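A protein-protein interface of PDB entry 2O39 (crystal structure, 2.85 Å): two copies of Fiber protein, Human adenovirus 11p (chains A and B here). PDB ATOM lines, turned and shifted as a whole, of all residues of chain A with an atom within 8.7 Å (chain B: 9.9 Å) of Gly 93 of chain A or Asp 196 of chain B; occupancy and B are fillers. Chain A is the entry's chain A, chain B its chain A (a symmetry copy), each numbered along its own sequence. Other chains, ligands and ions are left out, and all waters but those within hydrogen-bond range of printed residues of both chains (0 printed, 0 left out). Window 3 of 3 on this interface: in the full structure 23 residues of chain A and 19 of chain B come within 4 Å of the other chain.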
ATOM      1  N   ASN A   2      14.083  15.192 -10.664  1.00  0.00           N
ATOM      2  CA  ASN A   2      14.571  13.941 -10.086  1.00  0.00           C
ATOM      3  C   ASN A   2      14.280  13.918  -8.594  1.00  0.00           C
ATOM      4  O   ASN A   2      14.934  13.191  -7.849  1.00  0.00           O
ATOM      5  CB  ASN A   2      16.095  13.818 -10.249  1.00  0.00           C
ATOM      6  CG  ASN A   2      16.591  14.253 -11.620  1.00  0.00           C
ATOM      7  OD1 ASN A   2      16.519  15.429 -11.981  1.00  0.00           O
ATOM      8  ND2 ASN A   2      17.111  13.300 -12.386  1.00  0.00           N
ATOM      9  N   THR A   5      13.553  10.536  -6.444  1.00  0.00           N
ATOM     10  CA  THR A   5      14.578   9.625  -5.950  1.00  0.00           C
ATOM     11  C   THR A   5      15.377  10.257  -4.815  1.00  0.00           C
ATOM     12  O   THR A   5      15.862  11.382  -4.937  1.00  0.00           O
ATOM     13  CB  THR A   5      15.545   9.200  -7.072  1.00  0.00           C
ATOM     14  OG1 THR A   5      14.795   8.756  -8.209  1.00  0.00           O
ATOM     15  CG2 THR A   5      16.451   8.074  -6.596  1.00  0.00           C
ATOM     16  N   TRP A   7      18.602   8.902  -2.940  1.00  0.00           N
ATOM     17  CA  TRP A   7      19.483   7.748  -3.087  1.00  0.00           C
ATOM     18  C   TRP A   7      20.921   8.103  -2.724  1.00  0.00           C
ATOM     19  O   TRP A   7      21.249   9.271  -2.520  1.00  0.00           O
ATOM     20  CB  TRP A   7      19.419   7.204  -4.515  1.00  0.00           C
ATOM     21  CG  TRP A   7      20.099   8.082  -5.522  1.00  0.00           C
ATOM     22  CD1 TRP A   7      20.469   9.384  -5.356  1.00  0.00           C
ATOM     23  CD2 TRP A   7      20.490   7.720  -6.852  1.00  0.00           C
ATOM     24  NE1 TRP A   7      21.066   9.857  -6.500  1.00  0.00           N
ATOM     25  CE2 TRP A   7      21.092   8.853  -7.433  1.00  0.00           C
ATOM     26  CE3 TRP A   7      20.390   6.547  -7.607  1.00  0.00           C
ATOM     27  CZ2 TRP A   7      21.591   8.849  -8.734  1.00  0.00           C
ATOM     28  CZ3 TRP A   7      20.887   6.545  -8.898  1.00  0.00           C
ATOM     29  CH2 TRP A   7      21.479   7.689  -9.448  1.00  0.00           C
ATOM     30  N   GLY A   9      23.405   7.653  -4.653  1.00  0.00           N
ATOM     31  CA  GLY A   9      24.122   7.903  -5.887  1.00  0.00           C
ATOM     32  C   GLY A   9      24.747   6.586  -6.311  1.00  0.00           C
ATOM     33  O   GLY A   9      24.956   5.706  -5.481  1.00  0.00           O
ATOM     34  N   VAL A  10      25.058   6.437  -7.591  1.00  0.00           N
ATOM     35  CA  VAL A  10      25.645   5.197  -8.079  1.00  0.00           C
ATOM     36  C   VAL A  10      27.104   5.033  -7.663  1.00  0.00           C
ATOM     37  O   VAL A  10      27.862   6.011  -7.603  1.00  0.00           O
ATOM     38  CB  VAL A  10      25.556   5.121  -9.608  1.00  0.00           C
ATOM     39  CG1 VAL A  10      26.004   3.757 -10.091  1.00  0.00           C
ATOM     40  CG2 VAL A  10      24.144   5.396 -10.047  1.00  0.00           C
ATOM     41  N   HIS A  90      18.696  13.839  -3.833  1.00  0.00           N
ATOM     42  CA  HIS A  90      17.947  13.589  -5.058  1.00  0.00           C
ATOM     43  C   HIS A  90      18.871  13.158  -6.192  1.00  0.00           C
ATOM     44  O   HIS A  90      20.094  13.251  -6.079  1.00  0.00           O
ATOM     45  CB  HIS A  90      17.159  14.836  -5.468  1.00  0.00           C
ATOM     46  CG  HIS A  90      15.974  15.115  -4.597  1.00  0.00           C
ATOM     47  ND1 HIS A  90      15.548  16.393  -4.309  1.00  0.00           N
ATOM     48  CD2 HIS A  90      15.126  14.281  -3.950  1.00  0.00           C
ATOM     49  CE1 HIS A  90      14.488  16.335  -3.522  1.00  0.00           C
ATOM     50  NE2 HIS A  90      14.212  15.065  -3.289  1.00  0.00           N
ATOM     51  N   LYS A  91      18.280  12.683  -7.283  1.00  0.00           N
ATOM     52  CA  LYS A  91      19.049  12.216  -8.430  1.00  0.00           C
ATOM     53  C   LYS A  91      19.682  13.382  -9.182  1.00  0.00           C
ATOM     54  O   LYS A  91      19.035  14.401  -9.422  1.00  0.00           O
ATOM     55  CB  LYS A  91      18.163  11.401  -9.373  1.00  0.00           C
ATOM     56  CG  LYS A  91      18.855  10.964 -10.654  1.00  0.00           C
ATOM     57  CD  LYS A  91      17.908  10.194 -11.559  1.00  0.00           C
ATOM     58  CE  LYS A  91      18.563   9.864 -12.891  1.00  0.00           C
ATOM     59  NZ  LYS A  91      19.620   8.825 -12.747  1.00  0.00           N
ATOM     60  N   SER A  92      20.948  13.224  -9.552  1.00  0.00           N
ATOM     61  CA  SER A  92      21.614  14.176 -10.433  1.00  0.00           C
ATOM     62  C   SER A  92      22.657  13.485 -11.304  1.00  0.00           C
ATOM     63  O   SER A  92      23.795  13.279 -10.882  1.00  0.00           O
ATOM     64  CB  SER A  92      22.267  15.295  -9.619  1.00  0.00           C
ATOM     65  OG  SER A  92      22.959  16.200 -10.460  1.00  0.00           O
ATOM     66  N   GLY A  93      22.262  13.129 -12.522  1.00  0.00           N
ATOM     67  CA  GLY A  93      22.843  11.991 -13.210  1.00  0.00           C
ATOM     68  C   GLY A  93      23.007  10.787 -12.304  1.00  0.00           C
ATOM     69  O   GLY A  93      22.069  10.383 -11.617  1.00  0.00           O
ATOM     70  N   GLN A  94      24.205  10.211 -12.304  1.00  0.00           N
ATOM     71  CA  GLN A  94      24.469   8.993 -11.547  1.00  0.00           C
ATOM     72  C   GLN A  94      24.913   9.314 -10.124  1.00  0.00           C
ATOM     73  O   GLN A  94      25.423   8.449  -9.412  1.00  0.00           O
ATOM     74  CB  GLN A  94      25.531   8.146 -12.250  1.00  0.00           C
ATOM     75  CG  GLN A  94      25.186   7.784 -13.685  1.00  0.00           C
ATOM     76  CD  GLN A  94      24.108   6.722 -13.776  1.00  0.00           C
ATOM     77  OE1 GLN A  94      22.917   7.022 -13.695  1.00  0.00           O
ATOM     78  NE2 GLN A  94      24.521   5.472 -13.945  1.00  0.00           N
ATOM     79  N   ASN A  95      24.715  10.564  -9.715  1.00  0.00           N
ATOM     80  CA  ASN A  95      25.257  11.052  -8.453  1.00  0.00           C
ATOM     81  C   ASN A  95      24.189  11.697  -7.577  1.00  0.00           C
ATOM     82  O   ASN A  95      23.060  11.914  -8.017  1.00  0.00           O
ATOM     83  CB  ASN A  95      26.396  12.041  -8.707  1.00  0.00           C
ATOM     84  CG  ASN A  95      27.504  11.450  -9.556  1.00  0.00           C
ATOM     85  OD1 ASN A  95      28.001  10.359  -9.276  1.00  0.00           O
ATOM     86  ND2 ASN A  95      27.896  12.168 -10.602  1.00  0.00           N
ATOM     87  N   MET A  96      24.552  12.000  -6.335  1.00  0.00           N
ATOM     88  CA  MET A  96      23.653  12.680  -5.423  1.00  0.00           C
ATOM     89  C   MET A  96      23.668  14.162  -5.748  1.00  0.00           C
ATOM     90  O   MET A  96      24.719  14.743  -6.017  1.00  0.00           O
ATOM     91  CB  MET A  96      24.093  12.466  -3.977  1.00  0.00           C
ATOM     92  CG  MET A  96      23.937  11.038  -3.490  1.00  0.00           C
ATOM     93  SD  MET A  96      24.500  10.827  -1.784  1.00  0.00           S
ATOM     94  CE  MET A  96      26.259  10.884  -2.005  1.00  0.00           C
ATOM     95  N   ALA A  97      22.489  14.764  -5.751  1.00  0.00           N
ATOM     96  CA  ALA A  97      22.371  16.182  -6.024  1.00  0.00           C
ATOM     97  C   ALA A  97      22.984  16.887  -4.828  1.00  0.00           C
ATOM     98  O   ALA A  97      23.306  16.248  -3.832  1.00  0.00           O
ATOM     99  CB  ALA A  97      20.909  16.560  -6.170  1.00  0.00           C
ATOM    100  N   LYS B  36      10.069   3.591 -16.683  1.00  0.00           N
ATOM    101  CA  LYS B  36      10.908   4.509 -15.944  1.00  0.00           C
ATOM    102  C   LYS B  36      10.249   4.863 -14.631  1.00  0.00           C
ATOM    103  O   LYS B  36       9.201   5.515 -14.596  1.00  0.00           O
ATOM    104  CB  LYS B  36      11.176   5.782 -16.739  1.00  0.00           C
ATOM    105  CG  LYS B  36      12.067   5.561 -17.935  1.00  0.00           C
ATOM    106  CD  LYS B  36      12.606   6.864 -18.469  1.00  0.00           C
ATOM    107  CE  LYS B  36      13.495   6.605 -19.663  1.00  0.00           C
ATOM    108  NZ  LYS B  36      14.219   7.831 -20.103  1.00  0.00           N
ATOM    109  N   GLY B  38      11.671   6.503 -11.279  1.00  0.00           N
ATOM    110  CA  GLY B  38      12.751   7.099 -10.515  1.00  0.00           C
ATOM    111  C   GLY B  38      14.070   6.843 -11.193  1.00  0.00           C
ATOM    112  O   GLY B  38      14.108   6.717 -12.407  1.00  0.00           O
ATOM    113  N   ALA B  39      15.144   6.763 -10.414  1.00  0.00           N
ATOM    114  CA  ALA B  39      16.475   6.517 -10.952  1.00  0.00           C
ATOM    115  C   ALA B  39      16.615   5.059 -11.376  1.00  0.00           C
ATOM    116  O   ALA B  39      17.685   4.630 -11.824  1.00  0.00           O
ATOM    117  CB  ALA B  39      17.531   6.864  -9.915  1.00  0.00           C
ATOM    118  N   LEU B  40      15.524   4.307 -11.240  1.00  0.00           N
ATOM    119  CA  LEU B  40      15.504   2.899 -11.614  1.00  0.00           C
ATOM    120  C   LEU B  40      14.590   2.598 -12.808  1.00  0.00           C
ATOM    121  O   LEU B  40      13.801   3.436 -13.260  1.00  0.00           O
ATOM    122  CB  LEU B  40      15.010   2.053 -10.454  1.00  0.00           C
ATOM    123  CG  LEU B  40      15.649   2.206  -9.091  1.00  0.00           C
ATOM    124  CD1 LEU B  40      14.884   1.326  -8.123  1.00  0.00           C
ATOM    125  CD2 LEU B  40      17.106   1.824  -9.148  1.00  0.00           C
ATOM    126  N   VAL B  41      14.717   1.376 -13.313  1.00  0.00           N
ATOM    127  CA  VAL B  41      13.881   0.892 -14.391  1.00  0.00           C
ATOM    128  C   VAL B  41      13.256  -0.392 -13.859  1.00  0.00           C
ATOM    129  O   VAL B  41      13.936  -1.232 -13.259  1.00  0.00           O
ATOM    130  CB  VAL B  41      14.687   0.576 -15.671  1.00  0.00           C
ATOM    131  CG1 VAL B  41      13.854  -0.302 -16.611  1.00  0.00           C
ATOM    132  CG2 VAL B  41      15.047   1.869 -16.387  1.00  0.00           C
ATOM    133  N   SER B  73      24.365   2.632 -29.159  1.00  0.00           N
ATOM    134  CA  SER B  73      24.684   3.866 -28.450  1.00  0.00           C
ATOM    135  C   SER B  73      23.499   4.786 -28.146  1.00  0.00           C
ATOM    136  O   SER B  73      23.619   5.690 -27.324  1.00  0.00           O
ATOM    137  CB  SER B  73      25.719   4.639 -29.265  1.00  0.00           C
ATOM    138  OG  SER B  73      25.784   5.995 -28.882  1.00  0.00           O
ATOM    139  N   THR B  74      22.363   4.555 -28.792  1.00  0.00           N
ATOM    140  CA  THR B  74      21.191   5.404 -28.605  1.00  0.00           C
ATOM    141  C   THR B  74      20.050   4.766 -27.809  1.00  0.00           C
ATOM    142  O   THR B  74      19.108   5.455 -27.397  1.00  0.00           O
ATOM    143  CB  THR B  74      20.662   5.863 -29.975  1.00  0.00           C
ATOM    144  OG1 THR B  74      21.638   6.709 -30.589  1.00  0.00           O
ATOM    145  CG2 THR B  74      19.370   6.634 -29.838  1.00  0.00           C
ATOM    146  N   GLY B  75      20.135   3.454 -27.591  1.00  0.00           N
ATOM    147  CA  GLY B  75      19.104   2.752 -26.834  1.00  0.00           C
ATOM    148  C   GLY B  75      18.175   1.947 -27.719  1.00  0.00           C
ATOM    149  O   GLY B  75      17.109   1.520 -27.285  1.00  0.00           O
ATOM    150  N   ASN B 103      13.826   9.394 -25.616  1.00  0.00           N
ATOM    151  CA  ASN B 103      14.802   9.061 -24.595  1.00  0.00           C
ATOM    152  C   ASN B 103      15.021   7.593 -24.294  1.00  0.00           C
ATOM    153  O   ASN B 103      14.991   7.184 -23.131  1.00  0.00           O
ATOM    154  CB  ASN B 103      14.481   9.795 -23.295  1.00  0.00           C
ATOM    155  CG  ASN B 103      14.898  11.239 -23.347  1.00  0.00           C
ATOM    156  OD1 ASN B 103      14.108  12.114 -23.692  1.00  0.00           O
ATOM    157  ND2 ASN B 103      16.163  11.496 -23.035  1.00  0.00           N
ATOM    158  N   ALA B 104      15.270   6.805 -25.334  1.00  0.00           N
ATOM    159  CA  ALA B 104      15.525   5.390 -25.137  1.00  0.00           C
ATOM    160  C   ALA B 104      16.680   5.167 -24.146  1.00  0.00           C
ATOM    161  O   ALA B 104      16.554   4.348 -23.239  1.00  0.00           O
ATOM    162  CB  ALA B 104      15.840   4.722 -26.465  1.00  0.00           C
ATOM    163  N   LYS B 105      17.791   5.886 -24.313  1.00  0.00           N
ATOM    164  CA  LYS B 105      18.936   5.732 -23.419  1.00  0.00           C
ATOM    165  C   LYS B 105      18.461   5.574 -21.994  1.00  0.00           C
ATOM    166  O   LYS B 105      18.914   4.686 -21.270  1.00  0.00           O
ATOM    167  CB  LYS B 105      19.861   6.949 -23.485  1.00  0.00           C
ATOM    168  CG  LYS B 105      21.034   6.805 -24.444  1.00  0.00           C
ATOM    169  CD  LYS B 105      22.360   7.135 -23.774  1.00  0.00           C
ATOM    170  CE  LYS B 105      22.411   8.569 -23.299  1.00  0.00           C
ATOM    171  NZ  LYS B 105      23.689   8.844 -22.565  1.00  0.00           N
ATOM    172  N   GLY B 106      17.537   6.452 -21.610  1.00  0.00           N
ATOM    173  CA  GLY B 106      16.981   6.442 -20.269  1.00  0.00           C
ATOM    174  C   GLY B 106      16.502   5.095 -19.750  1.00  0.00           C
ATOM    175  O   GLY B 106      16.402   4.910 -18.537  1.00  0.00           O
ATOM    176  N   PHE B 107      16.194   4.166 -20.652  1.00  0.00           N
ATOM    177  CA  PHE B 107      15.731   2.838 -20.265  1.00  0.00           C
ATOM    178  C   PHE B 107      16.855   1.802 -20.187  1.00  0.00           C
ATOM    179  O   PHE B 107      16.649   0.693 -19.688  1.00  0.00           O
ATOM    180  CB  PHE B 107      14.693   2.322 -21.258  1.00  0.00           C
ATOM    181  CG  PHE B 107      13.432   3.128 -21.303  1.00  0.00           C
ATOM    182  CD1 PHE B 107      13.377   4.314 -22.018  1.00  0.00           C
ATOM    183  CD2 PHE B 107      12.284   2.689 -20.644  1.00  0.00           C
ATOM    184  CE1 PHE B 107      12.193   5.048 -22.087  1.00  0.00           C
ATOM    185  CE2 PHE B 107      11.106   3.411 -20.706  1.00  0.00           C
ATOM    186  CZ  PHE B 107      11.058   4.594 -21.425  1.00  0.00           C
ATOM    187  N   MET B 108      18.036   2.157 -20.677  1.00  0.00           N
ATOM    188  CA  MET B 108      19.154   1.228 -20.688  1.00  0.00           C
ATOM    189  C   MET B 108      19.796   0.999 -19.318  1.00  0.00           C
ATOM    190  O   MET B 108      19.783   1.876 -18.452  1.00  0.00           O
ATOM    191  CB  MET B 108      20.215   1.728 -21.661  1.00  0.00           C
ATOM    192  CG  MET B 108      19.718   1.879 -23.082  1.00  0.00           C
ATOM    193  SD  MET B 108      19.137   0.335 -23.766  1.00  0.00           S
ATOM    194  CE  MET B 108      17.397   0.670 -23.933  1.00  0.00           C
ATOM    195  N   PRO B 109      20.368  -0.195 -19.101  1.00  0.00           N
ATOM    196  CA  PRO B 109      21.002  -0.465 -17.815  1.00  0.00           C
ATOM    197  C   PRO B 109      22.297   0.330 -17.707  1.00  0.00           C
ATOM    198  O   PRO B 109      23.262   0.060 -18.421  1.00  0.00           O
ATOM    199  CB  PRO B 109      21.244  -1.965 -17.866  1.00  0.00           C
ATOM    200  CG  PRO B 109      21.500  -2.201 -19.303  1.00  0.00           C
ATOM    201  CD  PRO B 109      20.436  -1.376 -19.974  1.00  0.00           C
ATOM    202  N   SER B 110      22.299   1.317 -16.815  1.00  0.00           N
ATOM    203  CA  SER B 110      23.464   2.175 -16.577  1.00  0.00           C
ATOM    204  C   SER B 110      24.816   1.484 -16.652  1.00  0.00           C
ATOM    205  O   SER B 110      25.042   0.469 -15.988  1.00  0.00           O
ATOM    206  CB  SER B 110      23.374   2.829 -15.208  1.00  0.00           C
ATOM    207  OG  SER B 110      24.671   3.213 -14.773  1.00  0.00           O
ATOM    208  N   THR B 111      25.720   2.053 -17.444  1.00  0.00           N
ATOM    209  CA  THR B 111      27.066   1.499 -17.565  1.00  0.00           C
ATOM    210  C   THR B 111      27.874   1.848 -16.312  1.00  0.00           C
ATOM    211  O   THR B 111      28.859   1.184 -16.008  1.00  0.00           O
ATOM    212  CB  THR B 111      27.785   2.045 -18.800  1.00  0.00           C
ATOM    213  OG1 THR B 111      27.637   3.466 -18.842  1.00  0.00           O
ATOM    214  CG2 THR B 111      27.197   1.444 -20.070  1.00  0.00           C
ATOM    215  N   THR B 112      27.438   2.883 -15.591  1.00  0.00           N
ATOM    216  CA  THR B 112      28.095   3.313 -14.357  1.00  0.00           C
ATOM    217  C   THR B 112      27.843   2.279 -13.258  1.00  0.00           C
ATOM    218  O   THR B 112      28.749   1.914 -12.514  1.00  0.00           O
ATOM    219  CB  THR B 112      27.561   4.695 -13.871  1.00  0.00           C
ATOM    220  OG1 THR B 112      27.790   5.690 -14.876  1.00  0.00           O
ATOM    221  CG2 THR B 112      28.270   5.125 -12.595  1.00  0.00           C
ATOM    222  N   ALA B 113      26.603   1.816 -13.158  1.00  0.00           N
ATOM    223  CA  ALA B 113      26.236   0.820 -12.163  1.00  0.00           C
ATOM    224  C   ALA B 113      26.592  -0.599 -12.606  1.00  0.00           C
ATOM    225  O   ALA B 113      26.960  -1.434 -11.791  1.00  0.00           O
ATOM    226  CB  ALA B 113      24.779   0.907 -11.885  1.00  0.00           C
ATOM    227  N   TYR B 160      24.894  -1.452 -24.917  1.00  0.00           N
ATOM    228  CA  TYR B 160      24.249  -1.922 -23.687  1.00  0.00           C
ATOM    229  C   TYR B 160      23.793  -3.353 -23.929  1.00  0.00           C
ATOM    230  O   TYR B 160      23.618  -3.753 -25.078  1.00  0.00           O
ATOM    231  CB  TYR B 160      23.026  -1.071 -23.322  1.00  0.00           C
ATOM    232  CG  TYR B 160      23.286   0.407 -23.170  1.00  0.00           C
ATOM    233  CD1 TYR B 160      23.327   1.242 -24.283  1.00  0.00           C
ATOM    234  CD2 TYR B 160      23.483   0.977 -21.912  1.00  0.00           C
ATOM    235  CE1 TYR B 160      23.552   2.603 -24.154  1.00  0.00           C
ATOM    236  CE2 TYR B 160      23.714   2.348 -21.773  1.00  0.00           C
ATOM    237  CZ  TYR B 160      23.744   3.150 -22.900  1.00  0.00           C
ATOM    238  OH  TYR B 160      23.968   4.498 -22.781  1.00  0.00           O
ATOM    239  N   TYR B 192      16.859  -2.264 -11.908  1.00  0.00           N
ATOM    240  CA  TYR B 192      18.231  -1.877 -12.190  1.00  0.00           C
ATOM    241  C   TYR B 192      18.352  -0.377 -12.364  1.00  0.00           C
ATOM    242  O   TYR B 192      17.399   0.284 -12.778  1.00  0.00           O
ATOM    243  CB  TYR B 192      18.783  -2.619 -13.425  1.00  0.00           C
ATOM    244  CG  TYR B 192      18.142  -2.308 -14.778  1.00  0.00           C
ATOM    245  CD1 TYR B 192      18.296  -1.058 -15.383  1.00  0.00           C
ATOM    246  CD2 TYR B 192      17.414  -3.281 -15.470  1.00  0.00           C
ATOM    247  CE1 TYR B 192      17.741  -0.788 -16.645  1.00  0.00           C
ATOM    248  CE2 TYR B 192      16.857  -3.019 -16.725  1.00  0.00           C
ATOM    249  CZ  TYR B 192      17.022  -1.773 -17.305  1.00  0.00           C
ATOM    250  OH  TYR B 192      16.450  -1.504 -18.528  1.00  0.00           O
ATOM    251  N   ILE B 193      19.527   0.154 -12.012  1.00  0.00           N
ATOM    252  CA  ILE B 193      19.823   1.585 -12.131  1.00  0.00           C
ATOM    253  C   ILE B 193      19.895   1.889 -13.614  1.00  0.00           C
ATOM    254  O   ILE B 193      20.554   1.158 -14.354  1.00  0.00           O
ATOM    255  CB  ILE B 193      21.193   1.950 -11.536  1.00  0.00           C
ATOM    256  CG1 ILE B 193      21.299   1.471 -10.088  1.00  0.00           C
ATOM    257  CG2 ILE B 193      21.387   3.465 -11.601  1.00  0.00           C
ATOM    258  CD1 ILE B 193      20.351   2.163  -9.139  1.00  0.00           C
ATOM    259  N   ARG B 194      19.243   2.965 -14.044  1.00  0.00           N
ATOM    260  CA  ARG B 194      19.244   3.299 -15.460  1.00  0.00           C
ATOM    261  C   ARG B 194      20.314   4.294 -15.911  1.00  0.00           C
ATOM    262  O   ARG B 194      20.779   5.132 -15.142  1.00  0.00           O
ATOM    263  CB  ARG B 194      17.857   3.801 -15.880  1.00  0.00           C
ATOM    264  CG  ARG B 194      17.508   5.183 -15.408  1.00  0.00           C
ATOM    265  CD  ARG B 194      16.008   5.463 -15.521  1.00  0.00           C
ATOM    266  NE  ARG B 194      15.703   6.843 -15.144  1.00  0.00           N
ATOM    267  CZ  ARG B 194      15.675   7.858 -16.000  1.00  0.00           C
ATOM    268  NH1 ARG B 194      15.918   7.643 -17.287  1.00  0.00           N
ATOM    269  NH2 ARG B 194      15.444   9.088 -15.570  1.00  0.00           N
ATOM    270  N   GLU B 195      20.722   4.169 -17.166  1.00  0.00           N
ATOM    271  CA  GLU B 195      21.702   5.074 -17.732  1.00  0.00           C
ATOM    272  C   GLU B 195      21.012   6.432 -17.791  1.00  0.00           C
ATOM    273  O   GLU B 195      19.785   6.525 -17.697  1.00  0.00           O
ATOM    274  CB  GLU B 195      22.086   4.632 -19.147  1.00  0.00           C
ATOM    275  CG  GLU B 195      23.140   5.496 -19.813  1.00  0.00           C
ATOM    276  CD  GLU B 195      24.553   5.182 -19.337  1.00  0.00           C
ATOM    277  OE1 GLU B 195      24.881   5.469 -18.162  1.00  0.00           O
ATOM    278  OE2 GLU B 195      25.345   4.640 -20.151  1.00  0.00           O
ATOM    279  N   ASP B 196      21.796   7.490 -17.922  1.00  0.00           N
ATOM    280  CA  ASP B 196      21.215   8.810 -18.014  1.00  0.00           C
ATOM    281  C   ASP B 196      20.846   9.046 -19.455  1.00  0.00           C
ATOM    282  O   ASP B 196      21.453   8.471 -20.358  1.00  0.00           O
ATOM    283  CB  ASP B 196      22.213   9.857 -17.559  1.00  0.00           C
ATOM    284  CG  ASP B 196      22.216  10.028 -16.066  1.00  0.00           C
ATOM    285  OD1 ASP B 196      23.318  10.038 -15.470  1.00  0.00           O
ATOM    286  OD2 ASP B 196      21.104  10.160 -15.495  1.00  0.00           O
ATOM    287  N   ASP B 197      19.846   9.886 -19.674  1.00  0.00           N
ATOM    288  CA  ASP B 197      19.406  10.193 -21.029  1.00  0.00           C
ATOM    289  C   ASP B 197      20.536  10.918 -21.777  1.00  0.00           C
ATOM    290  O   ASP B 197      21.596  11.166 -21.155  1.00  0.00           O
ATOM    291  CB  ASP B 197      18.142  11.064 -20.975  1.00  0.00           C
ATOM    292  CG  ASP B 197      17.024  10.434 -20.136  1.00  0.00           C
ATOM    293  OD1 ASP B 197      17.245  10.174 -18.935  1.00  0.00           O
ATOM    294  OD2 ASP B 197      15.920  10.201 -20.671  1.00  0.00           O
ATOM    295  OXT ASP B 197      20.359  11.226 -22.977  1.00  0.00           O
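Hydrophobic or aromatic side chains of chain A within 4 Å of the printed part of chain B: Trp 7 and Val 10.
Among the printed residues, Asp or Glu carboxylates within 4 Å of a Lys or Arg side-chain nitrogen of the other chain: Lys 91 of chain A with Asp 196 of chain B.
The side-chain hydroxyl of Thr 5 of chain A sits at hydrogen-bond distance from the backbone NH of Ala 39 of chain B (3.0 Å).
OD2 of Asp 196 of chain B is in salt-bridge range of NZ of Lys 91 of chain A (3.4 Å).
NE2 of Gln 94 of chain A sits at hydrogen-bond distance from OG of Ser 110 of chain B, 2.4 Å away.
The side-chain hydroxyl (OG1) of Thr 112 of chain B sits close to the side-chain amide nitrogen (NE2) of Gln 94 of chain A, 3.4 Å away.
The side-chain amide oxygen (OE1) of Gln 94 of chain A sits close to the backbone carbonyl oxygen (O) of Arg 194 of chain B, 3.2 Å away.
N of Gln 94 of chain A sits at hydrogen-bond distance from OD1 of Asp 196 of chain B.
Among the printed residues, merely in contact across the chains: Gly 93 of chain A with Asp 196 of chain B (3.0 Å), Thr 5 of chain A with Gly 38 of chain B (3.5 Å), Trp 7 of chain A with Ala 39 of chain B (3.5 Å), Val 10 of chain A with Ala 113 of chain B (3.6 Å), Val 10 of chain A with Thr 112 of chain B (3.6 Å), Val 10 of chain A with Ile 193 of chain B (3.7 Å) and Lys 91 of chain A with Ala 39 of chain B (3.7 Å).
O of Asn 2 of chain A lies within hydrogen-bond range of N of Lys 91 of chain A (3.4 Å).
O of Asp 196 of chain B sits close to NZ of Lys 105 of chain B (3.2 Å).
O of Gly 106 of chain B lies within hydrogen-bond range of NH1 of Arg 194 of chain B (3.0 Å).
The side-chain hydroxyl of Ser 110 of chain B lies within hydrogen-bond range of the backbone NH of Ala 113 of chain B.
The backbone carbonyl oxygen (O) of Ile 193 of chain B sits at hydrogen-bond distance from the backbone NH (N) of Ser 110 of chain B.
NH1 of Arg 194 of chain B is in salt-bridge range of OD1 of Asp 197 of chain B (3.3 Å).
No position is printed for both chains.
Of the 13 pairs that touch across the chains among the printed residues, none has its exchanged pair printed and touching as well.
Printed residues of chain B within 4 Å of Trp 7 of chain A: Ala 39.
Of the printed residues of chain B, Val 10 of chain A touches Thr 112, Ala 113 and Ile 193.
His 90 of chain A touches none of the printed residues of chain B.
No residue of chain B comes within 4 Å of Ser 92 of chain A.
Of the printed residues of chain B, Gly 93 of chain A touches Asp 196 (3.0 Å).
Of chain B, only Ser 110 (2.4 Å), Thr 112 (3.1 Å), Arg 194 (3.2 Å) and Asp 196 (3.3 Å) come within 4 Å of Gln 94 of chain A.
Lys 105 of chain B touches none of the printed residues of chain A.
Printed residues of chain A within 4 Å of Ile 193 of chain B: Val 10.
Of the printed residues of chain A, Arg 194 of chain B touches Gln 94.
Of chain A, only Lys 91, Gly 93 and Gln 94 come within 4 Å of Asp 196 of chain B.
The nearest residue of chain A that does not touch Asp 196 of chain B is Ser 92 of chain A (5.4 Å).
The nearest printed residue of chain A that does not touch Gly 38 of chain B is Lys 91 of chain A (5.1 Å).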
